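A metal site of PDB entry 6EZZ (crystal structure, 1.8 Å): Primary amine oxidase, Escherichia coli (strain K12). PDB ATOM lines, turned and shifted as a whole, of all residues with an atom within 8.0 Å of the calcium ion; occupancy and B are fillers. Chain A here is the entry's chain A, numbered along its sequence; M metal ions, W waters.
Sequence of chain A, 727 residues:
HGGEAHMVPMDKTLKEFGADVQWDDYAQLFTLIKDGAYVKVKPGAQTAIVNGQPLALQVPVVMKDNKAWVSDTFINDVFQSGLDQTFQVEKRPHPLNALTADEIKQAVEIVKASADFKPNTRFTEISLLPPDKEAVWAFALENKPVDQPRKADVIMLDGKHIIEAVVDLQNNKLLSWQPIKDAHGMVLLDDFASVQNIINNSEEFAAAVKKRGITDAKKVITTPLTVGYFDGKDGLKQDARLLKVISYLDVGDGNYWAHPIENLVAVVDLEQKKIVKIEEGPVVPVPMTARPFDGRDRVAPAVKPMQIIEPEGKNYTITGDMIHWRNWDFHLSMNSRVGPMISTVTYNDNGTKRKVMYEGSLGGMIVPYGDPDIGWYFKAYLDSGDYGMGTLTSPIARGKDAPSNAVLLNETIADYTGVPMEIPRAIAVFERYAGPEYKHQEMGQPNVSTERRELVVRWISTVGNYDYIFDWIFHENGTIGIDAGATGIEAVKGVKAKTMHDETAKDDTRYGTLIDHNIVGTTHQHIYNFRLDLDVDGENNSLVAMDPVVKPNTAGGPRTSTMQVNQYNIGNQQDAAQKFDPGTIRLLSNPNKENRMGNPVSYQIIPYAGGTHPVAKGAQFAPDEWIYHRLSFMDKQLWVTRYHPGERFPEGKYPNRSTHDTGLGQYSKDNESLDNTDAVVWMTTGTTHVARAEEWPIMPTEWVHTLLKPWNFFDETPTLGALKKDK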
ATOM      1  N   LYS A 133     -13.746 -17.066  21.106  1.00  0.00           N
ATOM      2  CA  LYS A 133     -15.076 -17.117  20.478  1.00  0.00           C
ATOM      3  C   LYS A 133     -16.175 -16.484  21.335  1.00  0.00           C
ATOM      4  O   LYS A 133     -16.994 -15.719  20.836  1.00  0.00           O
ATOM      5  CB  LYS A 133     -15.420 -18.551  20.092  1.00  0.00           C
ATOM      6  CG  LYS A 133     -16.907 -18.808  19.795  1.00  0.00           C
ATOM      7  CD  LYS A 133     -17.081 -20.194  19.213  1.00  0.00           C
ATOM      8  CE  LYS A 133     -18.503 -20.405  18.705  1.00  0.00           C
ATOM      9  NZ  LYS A 133     -18.639 -21.692  18.000  1.00  0.00           N
ATOM     10  N   TRP A 137     -18.472 -13.231  20.087  1.00  0.00           N
ATOM     11  CA  TRP A 137     -19.913 -13.195  20.056  1.00  0.00           C
ATOM     12  C   TRP A 137     -20.488 -12.080  20.931  1.00  0.00           C
ATOM     13  O   TRP A 137     -21.498 -11.467  20.546  1.00  0.00           O
ATOM     14  CB  TRP A 137     -20.593 -14.526  20.460  1.00  0.00           C
ATOM     15  CG  TRP A 137     -20.880 -15.497  19.372  1.00  0.00           C
ATOM     16  CD1 TRP A 137     -20.569 -16.803  19.371  1.00  0.00           C
ATOM     17  CD2 TRP A 137     -21.615 -15.259  18.163  1.00  0.00           C
ATOM     18  NE1 TRP A 137     -21.047 -17.414  18.248  1.00  0.00           N
ATOM     19  CE2 TRP A 137     -21.692 -16.490  17.473  1.00  0.00           C
ATOM     20  CE3 TRP A 137     -22.201 -14.126  17.584  1.00  0.00           C
ATOM     21  CZ2 TRP A 137     -22.290 -16.616  16.231  1.00  0.00           C
ATOM     22  CZ3 TRP A 137     -22.815 -14.248  16.349  1.00  0.00           C
ATOM     23  CH2 TRP A 137     -22.847 -15.500  15.681  1.00  0.00           C
ATOM     24  N   VAL A 356     -26.515 -17.754  13.831  1.00  0.00           N
ATOM     25  CA  VAL A 356     -26.576 -18.816  12.820  1.00  0.00           C
ATOM     26  C   VAL A 356     -25.198 -19.442  12.647  1.00  0.00           C
ATOM     27  O   VAL A 356     -25.070 -20.669  12.694  1.00  0.00           O
ATOM     28  CB  VAL A 356     -27.109 -18.270  11.480  1.00  0.00           C
ATOM     29  CG1 VAL A 356     -27.068 -19.335  10.369  1.00  0.00           C
ATOM     30  CG2 VAL A 356     -28.500 -17.735  11.663  1.00  0.00           C
ATOM     31  N   MET A 357     -24.167 -18.632  12.426  1.00  0.00           N
ATOM     32  CA  MET A 357     -22.837 -19.165  12.139  1.00  0.00           C
ATOM     33  C   MET A 357     -21.719 -18.301  12.698  1.00  0.00           C
ATOM     34  O   MET A 357     -21.636 -17.112  12.389  1.00  0.00           O
ATOM     35  CB  MET A 357     -22.672 -19.391  10.616  1.00  0.00           C
ATOM     36  CG  MET A 357     -21.342 -19.992  10.253  1.00  0.00           C
ATOM     37  SD  MET A 357     -21.169 -20.493   8.498  1.00  0.00           S
ATOM     38  CE  MET A 357     -21.174 -18.900   7.710  1.00  0.00           C
ATOM     39  N   TYR A 358     -20.849 -18.897  13.526  1.00  0.00           N
ATOM     40  CA  TYR A 358     -19.697 -18.168  14.052  1.00  0.00           C
ATOM     41  C   TYR A 358     -18.663 -17.891  13.007  1.00  0.00           C
ATOM     42  O   TYR A 358     -18.195 -16.766  12.916  1.00  0.00           O
ATOM     43  CB  TYR A 358     -19.074 -18.875  15.268  1.00  0.00           C
ATOM     44  CG  TYR A 358     -17.917 -18.103  15.825  1.00  0.00           C
ATOM     45  CD1 TYR A 358     -18.110 -16.856  16.420  1.00  0.00           C
ATOM     46  CD2 TYR A 358     -16.626 -18.561  15.712  1.00  0.00           C
ATOM     47  CE1 TYR A 358     -17.043 -16.095  16.862  1.00  0.00           C
ATOM     48  CE2 TYR A 358     -15.536 -17.825  16.184  1.00  0.00           C
ATOM     49  CZ  TYR A 358     -15.762 -16.587  16.756  1.00  0.00           C
ATOM     50  OH  TYR A 358     -14.687 -15.837  17.191  1.00  0.00           O
ATOM     51  N   GLU A 359     -18.276 -18.888  12.221  1.00  0.00           N
ATOM     52  CA  GLU A 359     -17.261 -18.714  11.169  1.00  0.00           C
ATOM     53  C   GLU A 359     -17.537 -19.757  10.121  1.00  0.00           C
ATOM     54  O   GLU A 359     -17.759 -20.935  10.449  1.00  0.00           O
ATOM     55  CB  GLU A 359     -15.825 -19.000  11.647  1.00  0.00           C
ATOM     56  CG  GLU A 359     -15.230 -17.943  12.540  1.00  0.00           C
ATOM     57  CD  GLU A 359     -13.826 -18.296  13.062  1.00  0.00           C
ATOM     58  OE1 GLU A 359     -13.626 -19.321  13.766  1.00  0.00           O
ATOM     59  OE2 GLU A 359     -12.923 -17.477  12.799  1.00  0.00           O
ATOM     60  N   ARG A 531     -15.671 -25.535   5.830  1.00  0.00           N
ATOM     61  CA  ARG A 531     -15.700 -25.598   7.300  1.00  0.00           C
ATOM     62  C   ARG A 531     -16.693 -24.593   7.798  1.00  0.00           C
ATOM     63  O   ARG A 531     -16.502 -23.352   7.596  1.00  0.00           O
ATOM     64  CB  ARG A 531     -14.334 -25.284   7.877  1.00  0.00           C
ATOM     65  CG  ARG A 531     -14.316 -25.257   9.404  1.00  0.00           C
ATOM     66  CD  ARG A 531     -12.959 -24.872   9.973  1.00  0.00           C
ATOM     67  NE  ARG A 531     -12.998 -24.798  11.459  1.00  0.00           N
ATOM     68  CZ  ARG A 531     -13.587 -23.862  12.189  1.00  0.00           C
ATOM     69  NH1 ARG A 531     -14.183 -22.792  11.645  1.00  0.00           N
ATOM     70  NH2 ARG A 531     -13.561 -23.985  13.515  1.00  0.00           N
ATOM     71  N   LEU A 532     -17.749 -25.091   8.457  1.00  0.00           N
ATOM     72  CA  LEU A 532     -18.884 -24.270   8.835  1.00  0.00           C
ATOM     73  C   LEU A 532     -19.179 -24.418  10.329  1.00  0.00           C
ATOM     74  O   LEU A 532     -19.849 -25.389  10.748  1.00  0.00           O
ATOM     75  CB  LEU A 532     -20.112 -24.642   8.001  1.00  0.00           C
ATOM     76  CG  LEU A 532     -19.869 -24.636   6.472  1.00  0.00           C
ATOM     77  CD1 LEU A 532     -21.056 -25.292   5.778  1.00  0.00           C
ATOM     78  CD2 LEU A 532     -19.673 -23.192   5.991  1.00  0.00           C
ATOM     79  N   ASP A 533     -18.670 -23.500  11.130  1.00  0.00           N
ATOM     80  CA  ASP A 533     -18.974 -23.458  12.564  1.00  0.00           C
ATOM     81  C   ASP A 533     -20.322 -22.816  12.780  1.00  0.00           C
ATOM     82  O   ASP A 533     -20.440 -21.684  13.227  1.00  0.00           O
ATOM     83  CB  ASP A 533     -17.866 -22.734  13.324  1.00  0.00           C
ATOM     84  CG  ASP A 533     -18.106 -22.714  14.846  1.00  0.00           C
ATOM     85  OD1 ASP A 533     -18.988 -23.431  15.326  1.00  0.00           O
ATOM     86  OD2 ASP A 533     -17.381 -21.995  15.531  1.00  0.00           O
ATOM     87  N   LEU A 534     -21.365 -23.580  12.456  1.00  0.00           N
ATOM     88  CA  LEU A 534     -22.743 -23.224  12.718  1.00  0.00           C
ATOM     89  C   LEU A 534     -22.963 -23.228  14.239  1.00  0.00           C
ATOM     90  O   LEU A 534     -22.456 -24.090  14.916  1.00  0.00           O
ATOM     91  CB  LEU A 534     -23.708 -24.242  12.095  1.00  0.00           C
ATOM     92  CG  LEU A 534     -23.658 -24.365  10.561  1.00  0.00           C
ATOM     93  CD1 LEU A 534     -24.643 -25.397  10.053  1.00  0.00           C
ATOM     94  CD2 LEU A 534     -23.902 -23.004   9.932  1.00  0.00           C
ATOM     95  N   ASP A 535     -23.701 -22.243  14.748  1.00  0.00           N
ATOM     96  CA  ASP A 535     -24.080 -22.117  16.140  1.00  0.00           C
ATOM     97  C   ASP A 535     -25.567 -21.822  15.985  1.00  0.00           C
ATOM     98  O   ASP A 535     -25.951 -20.701  15.886  1.00  0.00           O
ATOM     99  CB  ASP A 535     -23.383 -20.936  16.797  1.00  0.00           C
ATOM    100  CG  ASP A 535     -21.972 -21.241  17.246  1.00  0.00           C
ATOM    101  OD1 ASP A 535     -21.490 -22.341  17.135  1.00  0.00           O
ATOM    102  OD2 ASP A 535     -21.346 -20.317  17.718  1.00  0.00           O
ATOM    103  N   VAL A 536     -26.379 -22.865  15.922  1.00  0.00           N
ATOM    104  CA  VAL A 536     -27.801 -22.735  15.620  1.00  0.00           C
ATOM    105  C   VAL A 536     -28.571 -22.166  16.822  1.00  0.00           C
ATOM    106  O   VAL A 536     -28.918 -22.901  17.770  1.00  0.00           O
ATOM    107  CB  VAL A 536     -28.373 -24.065  15.122  1.00  0.00           C
ATOM    108  CG1 VAL A 536     -29.884 -23.994  14.906  1.00  0.00           C
ATOM    109  CG2 VAL A 536     -27.679 -24.476  13.817  1.00  0.00           C
ATOM    110  N   GLY A 538     -27.460 -20.596  19.108  1.00  0.00           N
ATOM    111  CA  GLY A 538     -26.669 -20.886  20.306  1.00  0.00           C
ATOM    112  C   GLY A 538     -25.576 -21.851  20.011  1.00  0.00           C
ATOM    113  O   GLY A 538     -25.595 -22.501  18.964  1.00  0.00           O
ATOM    114  N   GLU A 539     -24.646 -21.892  20.958  1.00  0.00           N
ATOM    115  CA  GLU A 539     -23.489 -22.737  20.975  1.00  0.00           C
ATOM    116  C   GLU A 539     -23.806 -24.232  20.983  1.00  0.00           C
ATOM    117  O   GLU A 539     -23.228 -25.004  20.200  1.00  0.00           O
ATOM    118  CB  GLU A 539     -22.666 -22.364  22.240  1.00  0.00           C
ATOM    119  CG  GLU A 539     -21.368 -23.150  22.377  1.00  0.00           C
ATOM    120  CD  GLU A 539     -20.714 -23.003  23.727  1.00  0.00           C
ATOM    121  OE1 GLU A 539     -21.189 -22.208  24.550  1.00  0.00           O
ATOM    122  OE2 GLU A 539     -19.706 -23.685  23.972  1.00  0.00           O
ATOM    123  N   ASN A 540     -24.693 -24.632  21.872  1.00  0.00           N
ATOM    124  CA  ASN A 540     -24.954 -26.043  22.190  1.00  0.00           C
ATOM    125  C   ASN A 540     -25.990 -26.693  21.276  1.00  0.00           C
ATOM    126  O   ASN A 540     -27.164 -26.347  21.331  1.00  0.00           O
ATOM    127  CB  ASN A 540     -25.336 -26.123  23.665  1.00  0.00           C
ATOM    128  CG  ASN A 540     -24.158 -25.750  24.544  1.00  0.00           C
ATOM    129  OD1 ASN A 540     -23.025 -26.083  24.251  1.00  0.00           O
ATOM    130  ND2 ASN A 540     -24.425 -25.013  25.569  1.00  0.00           N
ATOM    131  N   ASN A 541     -25.505 -27.564  20.411  1.00  0.00           N
ATOM    132  CA  ASN A 541     -26.274 -28.156  19.323  1.00  0.00           C
ATOM    133  C   ASN A 541     -26.074 -29.688  19.312  1.00  0.00           C
ATOM    134  O   ASN A 541     -25.143 -30.233  19.949  1.00  0.00           O
ATOM    135  CB  ASN A 541     -25.833 -27.566  17.958  1.00  0.00           C
ATOM    136  CG  ASN A 541     -26.087 -26.079  17.795  1.00  0.00           C
ATOM    137  OD1 ASN A 541     -25.533 -25.509  16.847  1.00  0.00           O
ATOM    138  ND2 ASN A 541     -26.929 -25.425  18.623  1.00  0.00           N
ATOM    139  N   LEU A 588     -28.623 -29.884  12.086  1.00  0.00           N
ATOM    140  CA  LEU A 588     -27.964 -29.445  13.321  1.00  0.00           C
ATOM    141  C   LEU A 588     -29.005 -28.714  14.120  1.00  0.00           C
ATOM    142  O   LEU A 588     -29.516 -27.654  13.716  1.00  0.00           O
ATOM    143  CB  LEU A 588     -26.742 -28.556  13.013  1.00  0.00           C
ATOM    144  CG  LEU A 588     -25.779 -28.326  14.158  1.00  0.00           C
ATOM    145  CD1 LEU A 588     -25.173 -29.645  14.641  1.00  0.00           C
ATOM    146  CD2 LEU A 588     -24.705 -27.336  13.731  1.00  0.00           C
ATOM    147  N   THR A 641     -17.554 -32.188  14.077  1.00  0.00           N
ATOM    148  CA  THR A 641     -16.496 -32.278  15.108  1.00  0.00           C
ATOM    149  C   THR A 641     -16.826 -31.292  16.207  1.00  0.00           C
ATOM    150  O   THR A 641     -17.719 -30.459  16.055  1.00  0.00           O
ATOM    151  CB  THR A 641     -15.105 -32.014  14.514  1.00  0.00           C
ATOM    152  OG1 THR A 641     -15.037 -30.690  13.940  1.00  0.00           O
ATOM    153  CG2 THR A 641     -14.757 -33.079  13.459  1.00  0.00           C
ATOM    154  N   ARG A 642     -16.118 -31.384  17.312  1.00  0.00           N
ATOM    155  CA  ARG A 642     -16.309 -30.452  18.424  1.00  0.00           C
ATOM    156  C   ARG A 642     -15.438 -29.213  18.134  1.00  0.00           C
ATOM    157  O   ARG A 642     -14.339 -29.348  17.713  1.00  0.00           O
ATOM    158  CB  ARG A 642     -15.929 -31.078  19.793  1.00  0.00           C
ATOM    159  CG  ARG A 642     -16.752 -32.270  20.203  1.00  0.00           C
ATOM    160  CD  ARG A 642     -16.236 -32.974  21.456  1.00  0.00           C
ATOM    161  NE  ARG A 642     -16.079 -32.078  22.575  1.00  0.00           N
ATOM    162  CZ  ARG A 642     -16.961 -31.890  23.545  1.00  0.00           C
ATOM    163  NH1 ARG A 642     -18.098 -32.562  23.571  1.00  0.00           N
ATOM    164  NH2 ARG A 642     -16.702 -31.052  24.496  1.00  0.00           N
ATOM    165  N   TYR A 643     -15.961 -28.026  18.352  1.00  0.00           N
ATOM    166  CA  TYR A 643     -15.260 -26.783  18.140  1.00  0.00           C
ATOM    167  C   TYR A 643     -13.874 -26.810  18.796  1.00  0.00           C
ATOM    168  O   TYR A 643     -13.776 -27.090  19.985  1.00  0.00           O
ATOM    169  CB  TYR A 643     -16.046 -25.584  18.703  1.00  0.00           C
ATOM    170  CG  TYR A 643     -15.261 -24.290  18.615  1.00  0.00           C
ATOM    171  CD1 TYR A 643     -14.976 -23.707  17.375  1.00  0.00           C
ATOM    172  CD2 TYR A 643     -14.710 -23.714  19.768  1.00  0.00           C
ATOM    173  CE1 TYR A 643     -14.200 -22.555  17.301  1.00  0.00           C
ATOM    174  CE2 TYR A 643     -13.962 -22.546  19.687  1.00  0.00           C
ATOM    175  CZ  TYR A 643     -13.686 -21.984  18.450  1.00  0.00           C
ATOM    176  OH  TYR A 643     -12.909 -20.845  18.411  1.00  0.00           O
ATOM    177  N   THR A 677     -23.544 -29.748  22.371  1.00  0.00           N
ATOM    178  CA  THR A 677     -22.228 -29.163  22.540  1.00  0.00           C
ATOM    179  C   THR A 677     -21.884 -28.310  21.292  1.00  0.00           C
ATOM    180  O   THR A 677     -22.640 -28.307  20.317  1.00  0.00           O
ATOM    181  CB  THR A 677     -21.177 -30.264  22.825  1.00  0.00           C
ATOM    182  OG1 THR A 677     -19.953 -29.672  23.259  1.00  0.00           O
ATOM    183  CG2 THR A 677     -20.931 -31.161  21.608  1.00  0.00           C
ATOM    184  N   ASP A 678     -20.781 -27.577  21.361  1.00  0.00           N
ATOM    185  CA  ASP A 678     -20.381 -26.701  20.261  1.00  0.00           C
ATOM    186  C   ASP A 678     -19.848 -27.544  19.103  1.00  0.00           C
ATOM    187  O   ASP A 678     -18.777 -28.111  19.214  1.00  0.00           O
ATOM    188  CB  ASP A 678     -19.352 -25.663  20.721  1.00  0.00           C
ATOM    189  CG  ASP A 678     -19.150 -24.535  19.685  1.00  0.00           C
ATOM    190  OD1 ASP A 678     -19.661 -24.663  18.528  1.00  0.00           O
ATOM    191  OD2 ASP A 678     -18.492 -23.518  20.034  1.00  0.00           O
ATOM    192  N   ALA A 679     -20.618 -27.626  18.012  1.00  0.00           N
ATOM    193  CA  ALA A 679     -20.251 -28.398  16.843  1.00  0.00           C
ATOM    194  C   ALA A 679     -19.742 -27.547  15.682  1.00  0.00           C
ATOM    195  O   ALA A 679     -20.177 -26.401  15.549  1.00  0.00           O
ATOM    196  CB  ALA A 679     -21.442 -29.203  16.353  1.00  0.00           C
ATOM    197  N   VAL A 680     -18.953 -28.203  14.827  1.00  0.00           N
ATOM    198  CA  VAL A 680     -18.444 -27.637  13.571  1.00  0.00           C
ATOM    199  C   VAL A 680     -18.783 -28.656  12.477  1.00  0.00           C
ATOM    200  O   VAL A 680     -18.460 -29.828  12.580  1.00  0.00           O
ATOM    201  CB  VAL A 680     -16.916 -27.342  13.614  1.00  0.00           C
ATOM    202  CG1 VAL A 680     -16.403 -26.851  12.263  1.00  0.00           C
ATOM    203  CG2 VAL A 680     -16.577 -26.310  14.674  1.00  0.00           C
ATOM    204  N   VAL A 681     -19.468 -28.170  11.442  1.00  0.00           N
ATOM    205  CA  VAL A 681     -19.874 -29.004  10.333  1.00  0.00           C
ATOM    206  C   VAL A 681     -18.870 -28.806   9.221  1.00  0.00           C
ATOM    207  O   VAL A 681     -18.479 -27.682   8.942  1.00  0.00           O
ATOM    208  CB  VAL A 681     -21.257 -28.564   9.844  1.00  0.00           C
ATOM    209  CG1 VAL A 681     -21.622 -29.264   8.520  1.00  0.00           C
ATOM    210  CG2 VAL A 681     -22.298 -28.861  10.924  1.00  0.00           C
HETATM  211 CA    CA M   1     -20.780 -24.397  16.497  1.00  0.00          CA
HETATM  212  O   HOH W   1     -22.689 -25.495  17.590  1.00  0.00           O
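The calcium ion is bound by the side-chain carboxylate (OD1) of Asp 535 (2.3 Å), the backbone carbonyl oxygen (O) of Ala 679 (2.3 Å), the backbone carbonyl oxygen (O) of Leu 534 (2.3 Å), the side-chain carboxylate (OD1) of Asp 678 (2.3 Å), the side-chain carboxylate (OD1) of Asp 533 (2.3 Å) and water W1 (2.5 Å).
OD2 of Asp 533 lies within salt-bridge range of NZ of Lys 133. The backbone NH (N) of Asp 533 sits at hydrogen-bond distance from the backbone carbonyl oxygen (O) of Glu 359 (2.8 Å). The side-chain carboxylate (OD2) of Asp 678 is in salt-bridge range of the side-chain amino group (NZ) of Lys 133 (2.7 Å). O of Asp 678 is in hydrogen-bond range of N of Tyr 643 (2.9 Å). The backbone carbonyl oxygen (O) of Asp 533 lies within hydrogen-bond range of the backbone NH (N) of Tyr 358, at 2.8 Å. The side-chain carboxylate (OD2) of Asp 535 sits at hydrogen-bond distance from the indole nitrogen (NE1) of Trp 137, 3.0 Å away. The side-chain amino group (NZ) of Lys 133 lies within salt-bridge range of the side-chain carboxylate (OD2) of Asp 535. The backbone carbonyl oxygen of Val 356 sits at hydrogen-bond distance from the backbone NH of Asp 535.
Lys 133 touches the calcium ion. Six residues have an atom within 4 Å of the calcium ion: Lys 133, Asp 533, Leu 534, Asp 535, Asp 678 and Ala 679. Along chain A the residues within 4 Å of the calcium ion span positions 133 to 679. The nearest printed residue that does not touch the calcium ion is Glu 539 (4.5 Å).
Water W1 lies within hydrogen-bond range of O of Glu 539 (2.7 Å), OD1 of Asn 541 (2.9 Å) and N of Ala 679 (3.0 Å).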
